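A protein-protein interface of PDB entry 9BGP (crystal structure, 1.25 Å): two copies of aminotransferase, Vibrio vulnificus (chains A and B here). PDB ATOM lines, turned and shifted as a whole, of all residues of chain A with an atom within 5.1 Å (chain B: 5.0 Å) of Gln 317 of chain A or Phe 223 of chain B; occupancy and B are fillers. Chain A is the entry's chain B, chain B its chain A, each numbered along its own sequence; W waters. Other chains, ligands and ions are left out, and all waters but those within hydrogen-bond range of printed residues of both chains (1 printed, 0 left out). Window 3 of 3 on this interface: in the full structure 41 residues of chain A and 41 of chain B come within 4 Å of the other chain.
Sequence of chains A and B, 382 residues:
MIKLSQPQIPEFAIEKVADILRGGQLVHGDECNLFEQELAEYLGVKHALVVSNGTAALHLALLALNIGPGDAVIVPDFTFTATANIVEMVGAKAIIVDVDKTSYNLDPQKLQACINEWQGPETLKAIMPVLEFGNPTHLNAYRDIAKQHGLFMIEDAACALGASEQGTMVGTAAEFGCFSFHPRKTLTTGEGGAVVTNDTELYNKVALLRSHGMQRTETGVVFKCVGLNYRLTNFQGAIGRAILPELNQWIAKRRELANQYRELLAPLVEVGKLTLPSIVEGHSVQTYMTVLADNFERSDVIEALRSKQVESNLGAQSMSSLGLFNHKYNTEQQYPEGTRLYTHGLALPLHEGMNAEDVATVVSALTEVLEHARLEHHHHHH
Of the printed residues of chain B, Thr 81 of chain A touches Phe 223. Gln 317 of chain A touches just one residue of chain B: Phe 223 (3.7 Å). Printed residues of chain B within 4 Å of Leu 324 of chain A: Lys 224 (3.8 Å) and Cys 225 (3.9 Å). Of the printed residues of chain A, His 212 of chain B touches Phe 80 (3.6 Å). Phe 223 of chain B touches just these residues of chain A: Thr 81 (3.4 Å) and Gln 317 (3.7 Å). Of the printed residues of chain A, Cys 225 of chain B touches Leu 324.
Hydrophobic or aromatic side chains of chain A within 4 Å of the printed part of chain B: Phe 80 and Leu 324. Of the 8 printed residues of chain B, 4 touch a printed residue of chain A. Along chain B the printed residues that touch a printed residue of chain A span positions 212 to 225. Among the printed residues, 5 pairs touch across the chains.
No position is printed for both chains.
Among the printed residues, pairs that only touch across the chains: Phe 80 of chain A with His 212 of chain B (3.6 Å), Thr 81 of chain A with Phe 223 of chain B (3.4 Å), Gln 317 of chain A with Phe 223 of chain B (3.7 Å), Leu 324 of chain A with Lys 224 of chain B (3.8 Å) and Leu 324 of chain A with Cys 225 of chain B (3.9 Å).
O of Gly 213 of chain B is in hydrogen-bond range of N of Lys 224 of chain B, 2.8 Å away. The backbone carbonyl oxygen (O) of Thr 79 of chain A lies within hydrogen-bond range of the backbone NH (N) of Gln 317 of chain A. The side-chain hydroxyl (OG1) of Thr 81 of chain A is in hydrogen-bond range of the side-chain amide oxygen (OE1) of Gln 317 of chain A (3.3 Å).
Water W1 lies within hydrogen-bond range of O of Leu 322 of chain A (2.7 Å) and O of Phe 223 of chain B (2.7 Å).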
ATOM      1  N   ASP A  77       8.779  14.690  -4.904  1.00  0.00           N
ATOM      2  CA  ASP A  77       7.377  14.553  -4.601  1.00  0.00           C
ATOM      3  C   ASP A  77       7.140  13.354  -3.681  1.00  0.00           C
ATOM      4  O   ASP A  77       6.246  13.394  -2.833  1.00  0.00           O
ATOM      5  CB  ASP A  77       6.528  14.406  -5.871  1.00  0.00           C
ATOM      6  CG  ASP A  77       5.052  14.357  -5.533  1.00  0.00           C
ATOM      7  OD1 ASP A  77       4.501  15.383  -5.095  1.00  0.00           O
ATOM      8  OD2 ASP A  77       4.448  13.261  -5.705  1.00  0.00           O
ATOM      9  N   PHE A  78       7.900  12.265  -3.877  1.00  0.00           N
ATOM     10  CA  PHE A  78       7.637  11.027  -3.164  1.00  0.00           C
ATOM     11  C   PHE A  78       8.670  10.876  -2.049  1.00  0.00           C
ATOM     12  O   PHE A  78       9.854  10.766  -2.340  1.00  0.00           O
ATOM     13  CB  PHE A  78       7.711   9.854  -4.134  1.00  0.00           C
ATOM     14  CG  PHE A  78       7.320   8.536  -3.524  1.00  0.00           C
ATOM     15  CD1 PHE A  78       8.263   7.541  -3.372  1.00  0.00           C
ATOM     16  CD2 PHE A  78       6.030   8.288  -3.089  1.00  0.00           C
ATOM     17  CE1 PHE A  78       7.920   6.315  -2.829  1.00  0.00           C
ATOM     18  CE2 PHE A  78       5.670   7.059  -2.551  1.00  0.00           C
ATOM     19  CZ  PHE A  78       6.633   6.084  -2.414  1.00  0.00           C
ATOM     20  N   THR A  79       8.213  10.983  -0.794  1.00  0.00           N
ATOM     21  CA  THR A  79       9.077  10.928   0.368  1.00  0.00           C
ATOM     22  C   THR A  79       8.183  10.894   1.599  1.00  0.00           C
ATOM     23  O   THR A  79       6.966  11.050   1.503  1.00  0.00           O
ATOM     24  CB  THR A  79      10.066  12.095   0.399  1.00  0.00           C
ATOM     25  OG1 THR A  79      10.927  11.878   1.511  1.00  0.00           O
ATOM     26  CG2 THR A  79       9.404  13.454   0.414  1.00  0.00           C
ATOM     27  N   PHE A  80       8.792  10.657   2.766  1.00  0.00           N
ATOM     28  CA  PHE A  80       8.087  10.923   4.000  1.00  0.00           C
ATOM     29  C   PHE A  80       7.943  12.443   4.163  1.00  0.00           C
ATOM     30  O   PHE A  80       8.849  13.211   3.819  1.00  0.00           O
ATOM     31  CB  PHE A  80       8.837  10.281   5.166  1.00  0.00           C
ATOM     32  CG  PHE A  80       8.122  10.440   6.470  1.00  0.00           C
ATOM     33  CD1 PHE A  80       8.661  11.220   7.487  1.00  0.00           C
ATOM     34  CD2 PHE A  80       6.866   9.896   6.651  1.00  0.00           C
ATOM     35  CE1 PHE A  80       7.978  11.400   8.676  1.00  0.00           C
ATOM     36  CE2 PHE A  80       6.175  10.097   7.837  1.00  0.00           C
ATOM     37  CZ  PHE A  80       6.736  10.844   8.849  1.00  0.00           C
ATOM     38  N   THR A  81       6.813  12.871   4.734  1.00  0.00           N
ATOM     39  CA  THR A  81       6.427  14.273   4.757  1.00  0.00           C
ATOM     40  C   THR A  81       7.462  15.148   5.469  1.00  0.00           C
ATOM     41  O   THR A  81       7.549  16.351   5.178  1.00  0.00           O
ATOM     42  CB  THR A  81       5.042  14.403   5.401  1.00  0.00           C
ATOM     43  OG1 THR A  81       4.227  13.430   4.739  1.00  0.00           O
ATOM     44  CG2 THR A  81       4.449  15.771   5.254  1.00  0.00           C
ATOM     45  N   LEU A 314       1.477   1.634   2.603  1.00  0.00           N
ATOM     46  CA  LEU A 314       2.069   2.527   1.627  1.00  0.00           C
ATOM     47  C   LEU A 314       3.533   2.727   2.009  1.00  0.00           C
ATOM     48  O   LEU A 314       3.916   2.528   3.161  1.00  0.00           O
ATOM     49  CB  LEU A 314       1.269   3.832   1.510  1.00  0.00           C
ATOM     50  CG  LEU A 314       1.512   4.927   2.541  1.00  0.00           C
ATOM     51  CD1 LEU A 314       0.606   6.116   2.220  1.00  0.00           C
ATOM     52  CD2 LEU A 314       1.270   4.442   3.956  1.00  0.00           C
ATOM     53  N   GLY A 315       4.360   3.049   1.014  1.00  0.00           N
ATOM     54  CA  GLY A 315       5.777   3.278   1.217  1.00  0.00           C
ATOM     55  C   GLY A 315       6.102   4.690   1.680  1.00  0.00           C
ATOM     56  O   GLY A 315       6.951   4.879   2.548  1.00  0.00           O
ATOM     57  N   ALA A 316       5.486   5.674   1.041  1.00  0.00           N
ATOM     58  CA  ALA A 316       5.728   7.078   1.370  1.00  0.00           C
ATOM     59  C   ALA A 316       4.583   7.918   0.828  1.00  0.00           C
ATOM     60  O   ALA A 316       3.632   7.371   0.239  1.00  0.00           O
ATOM     61  CB  ALA A 316       7.081   7.545   0.872  1.00  0.00           C
ATOM     62  N   GLN A 317       4.669   9.238   1.036  1.00  0.00           N
ATOM     63  CA  GLN A 317       3.628  10.159   0.644  1.00  0.00           C
ATOM     64  C   GLN A 317       3.976  10.869  -0.660  1.00  0.00           C
ATOM     65  O   GLN A 317       5.127  10.887  -1.103  1.00  0.00           O
ATOM     66  CB  GLN A 317       3.423  11.210   1.731  1.00  0.00           C
ATOM     67  CG  GLN A 317       2.779  10.644   2.994  1.00  0.00           C
ATOM     68  CD  GLN A 317       3.746   9.903   3.862  1.00  0.00           C
ATOM     69  OE1 GLN A 317       4.898  10.300   4.041  1.00  0.00           O
ATOM     70  NE2 GLN A 317       3.259   8.831   4.460  1.00  0.00           N
ATOM     71  N   SER A 318       2.949  11.484  -1.257  1.00  0.00           N
ATOM     72  CA  SER A 318       3.154  12.425  -2.359  1.00  0.00           C
ATOM     73  C   SER A 318       2.975  13.849  -1.831  1.00  0.00           C
ATOM     74  O   SER A 318       1.896  14.212  -1.372  1.00  0.00           O
ATOM     75  CB  SER A 318       2.171  12.158  -3.486  1.00  0.00           C
ATOM     76  OG  SER A 318       2.152  13.254  -4.414  1.00  0.00           O
ATOM     77  N   MET A 319       4.046  14.630  -1.806  1.00  0.00           N
ATOM     78  CA  MET A 319       4.003  15.955  -1.198  1.00  0.00           C
ATOM     79  C   MET A 319       2.962  16.838  -1.882  1.00  0.00           C
ATOM     80  O   MET A 319       2.255  17.598  -1.198  1.00  0.00           O
ATOM     81  CB  MET A 319       5.364  16.646  -1.298  1.00  0.00           C
ATOM     82  CG  MET A 319       6.503  15.915  -0.574  1.00  0.00           C
ATOM     83  SD  MET A 319       6.220  15.611   1.206  1.00  0.00           S
ATOM     84  CE  MET A 319       5.427  14.003   1.180  1.00  0.00           C
ATOM     85  N   LEU A 322      -0.694  16.603  -0.588  1.00  0.00           N
ATOM     86  CA  LEU A 322      -1.042  16.833   0.809  1.00  0.00           C
ATOM     87  C   LEU A 322      -1.657  18.214   1.032  1.00  0.00           C
ATOM     88  O   LEU A 322      -2.224  18.493   2.079  1.00  0.00           O
ATOM     89  CB  LEU A 322       0.240  16.706   1.649  1.00  0.00           C
ATOM     90  CG  LEU A 322       0.853  15.320   1.691  1.00  0.00           C
ATOM     91  CD1 LEU A 322       2.052  15.288   2.643  1.00  0.00           C
ATOM     92  CD2 LEU A 322      -0.182  14.292   2.109  1.00  0.00           C
ATOM     93  N   LEU A 324      -0.084  21.070   1.557  1.00  0.00           N
ATOM     94  CA  LEU A 324       0.708  21.790   2.546  1.00  0.00           C
ATOM     95  C   LEU A 324       1.789  22.667   1.923  1.00  0.00           C
ATOM     96  O   LEU A 324       2.336  23.527   2.608  1.00  0.00           O
ATOM     97  CB  LEU A 324       1.384  20.801   3.500  1.00  0.00           C
ATOM     98  CG  LEU A 324       0.446  19.916   4.300  1.00  0.00           C
ATOM     99  CD1 LEU A 324       1.275  18.986   5.156  1.00  0.00           C
ATOM    100  CD2 LEU A 324      -0.501  20.763   5.136  1.00  0.00           C
ATOM    101  N   TYR A 342       2.519   7.016  -4.375  1.00  0.00           N
ATOM    102  CA  TYR A 342       1.732   7.278  -3.181  1.00  0.00           C
ATOM    103  C   TYR A 342       0.424   6.505  -3.172  1.00  0.00           C
ATOM    104  O   TYR A 342       0.051   5.964  -2.134  1.00  0.00           O
ATOM    105  CB  TYR A 342       1.395   8.759  -3.139  1.00  0.00           C
ATOM    106  CG  TYR A 342       0.435   9.210  -2.079  1.00  0.00           C
ATOM    107  CD1 TYR A 342      -0.638  10.021  -2.415  1.00  0.00           C
ATOM    108  CD2 TYR A 342       0.634   8.900  -0.748  1.00  0.00           C
ATOM    109  CE1 TYR A 342      -1.451  10.567  -1.439  1.00  0.00           C
ATOM    110  CE2 TYR A 342      -0.183   9.424   0.240  1.00  0.00           C
ATOM    111  CZ  TYR A 342      -1.214  10.279  -0.114  1.00  0.00           C
ATOM    112  OH  TYR A 342      -2.022  10.810   0.859  1.00  0.00           O
ATOM    113  N   HIS B 212       5.143  15.709  12.959  1.00  0.00           N
ATOM    114  CA  HIS B 212       5.044  15.841  11.503  1.00  0.00           C
ATOM    115  C   HIS B 212       3.654  16.272  11.018  1.00  0.00           C
ATOM    116  O   HIS B 212       3.320  16.146   9.818  1.00  0.00           O
ATOM    117  CB  HIS B 212       5.441  14.547  10.776  1.00  0.00           C
ATOM    118  CG  HIS B 212       6.669  13.882  11.280  1.00  0.00           C
ATOM    119  ND1 HIS B 212       7.912  14.463  11.078  1.00  0.00           N
ATOM    120  CD2 HIS B 212       6.885  12.708  11.892  1.00  0.00           C
ATOM    121  CE1 HIS B 212       8.819  13.630  11.547  1.00  0.00           C
ATOM    122  NE2 HIS B 212       8.223  12.588  12.087  1.00  0.00           N
ATOM    123  N   GLY B 213       2.825  16.810  11.914  1.00  0.00           N
ATOM    124  CA  GLY B 213       1.454  17.166  11.562  1.00  0.00           C
ATOM    125  C   GLY B 213       0.509  15.981  11.445  1.00  0.00           C
ATOM    126  O   GLY B 213      -0.593  16.111  10.909  1.00  0.00           O
ATOM    127  N   MET B 214       0.924  14.817  11.928  1.00  0.00           N
ATOM    128  CA  MET B 214       0.153  13.588  11.776  1.00  0.00           C
ATOM    129  C   MET B 214      -1.052  13.570  12.717  1.00  0.00           C
ATOM    130  O   MET B 214      -0.915  13.770  13.921  1.00  0.00           O
ATOM    131  CB  MET B 214       1.040  12.383  12.092  1.00  0.00           C
ATOM    132  CG  MET B 214       2.121  12.160  11.077  1.00  0.00           C
ATOM    133  SD  MET B 214       3.465  11.013  11.655  1.00  0.00           S
ATOM    134  CE  MET B 214       2.572   9.460  11.720  1.00  0.00           C
ATOM    135  N   VAL B 221      -3.621   7.761   8.605  1.00  0.00           N
ATOM    136  CA  VAL B 221      -2.928   8.964   9.039  1.00  0.00           C
ATOM    137  C   VAL B 221      -3.182  10.054   8.003  1.00  0.00           C
ATOM    138  O   VAL B 221      -3.096   9.785   6.811  1.00  0.00           O
ATOM    139  CB  VAL B 221      -1.424   8.683   9.227  1.00  0.00           C
ATOM    140  CG1 VAL B 221      -0.594   9.959   9.286  1.00  0.00           C
ATOM    141  CG2 VAL B 221      -1.173   7.822  10.457  1.00  0.00           C
ATOM    142  N   VAL B 222      -3.482  11.274   8.474  1.00  0.00           N
ATOM    143  CA  VAL B 222      -3.559  12.465   7.638  1.00  0.00           C
ATOM    144  C   VAL B 222      -2.511  13.461   8.137  1.00  0.00           C
ATOM    145  O   VAL B 222      -2.306  13.564   9.348  1.00  0.00           O
ATOM    146  CB  VAL B 222      -4.968  13.078   7.696  1.00  0.00           C
ATOM    147  CG1 VAL B 222      -5.074  14.375   6.916  1.00  0.00           C
ATOM    148  CG2 VAL B 222      -6.025  12.089   7.218  1.00  0.00           C
ATOM    149  N   PHE B 223      -1.899  14.205   7.203  1.00  0.00           N
ATOM    150  CA  PHE B 223      -0.957  15.275   7.518  1.00  0.00           C
ATOM    151  C   PHE B 223      -1.699  16.608   7.504  1.00  0.00           C
ATOM    152  O   PHE B 223      -2.093  17.111   6.445  1.00  0.00           O
ATOM    153  CB  PHE B 223       0.230  15.231   6.547  1.00  0.00           C
ATOM    154  CG  PHE B 223       1.025  13.970   6.717  1.00  0.00           C
ATOM    155  CD1 PHE B 223       2.078  13.900   7.609  1.00  0.00           C
ATOM    156  CD2 PHE B 223       0.683  12.829   6.026  1.00  0.00           C
ATOM    157  CE1 PHE B 223       2.812  12.743   7.752  1.00  0.00           C
ATOM    158  CE2 PHE B 223       1.392  11.659   6.221  1.00  0.00           C
ATOM    159  CZ  PHE B 223       2.453  11.606   7.069  1.00  0.00           C
ATOM    160  N   LYS B 224      -1.971  17.173   8.687  1.00  0.00           N
ATOM    161  CA  LYS B 224      -2.823  18.336   8.802  1.00  0.00           C
ATOM    162  C   LYS B 224      -2.056  19.647   8.650  1.00  0.00           C
ATOM    163  O   LYS B 224      -2.631  20.672   8.274  1.00  0.00           O
ATOM    164  CB  LYS B 224      -3.524  18.291  10.156  1.00  0.00           C
ATOM    165  CG  LYS B 224      -4.728  17.371  10.194  1.00  0.00           C
ATOM    166  CD  LYS B 224      -5.725  17.692   9.085  1.00  0.00           C
ATOM    167  CE  LYS B 224      -7.021  16.918   9.175  1.00  0.00           C
ATOM    168  NZ  LYS B 224      -7.907  17.488  10.215  1.00  0.00           N
ATOM    169  N   CYS B 225      -0.758  19.645   8.955  1.00  0.00           N
ATOM    170  CA  CYS B 225       0.020  20.861   8.965  1.00  0.00           C
ATOM    171  C   CYS B 225       1.485  20.451   8.939  1.00  0.00           C
ATOM    172  O   CYS B 225       1.833  19.290   9.197  1.00  0.00           O
ATOM    173  CB  CYS B 225      -0.281  21.735  10.185  1.00  0.00           C
ATOM    174  SG  CYS B 225       0.165  20.979  11.777  1.00  0.00           S
HETATM  175  O   HOH W   1      -2.757  16.561   3.872  1.00  0.00           O
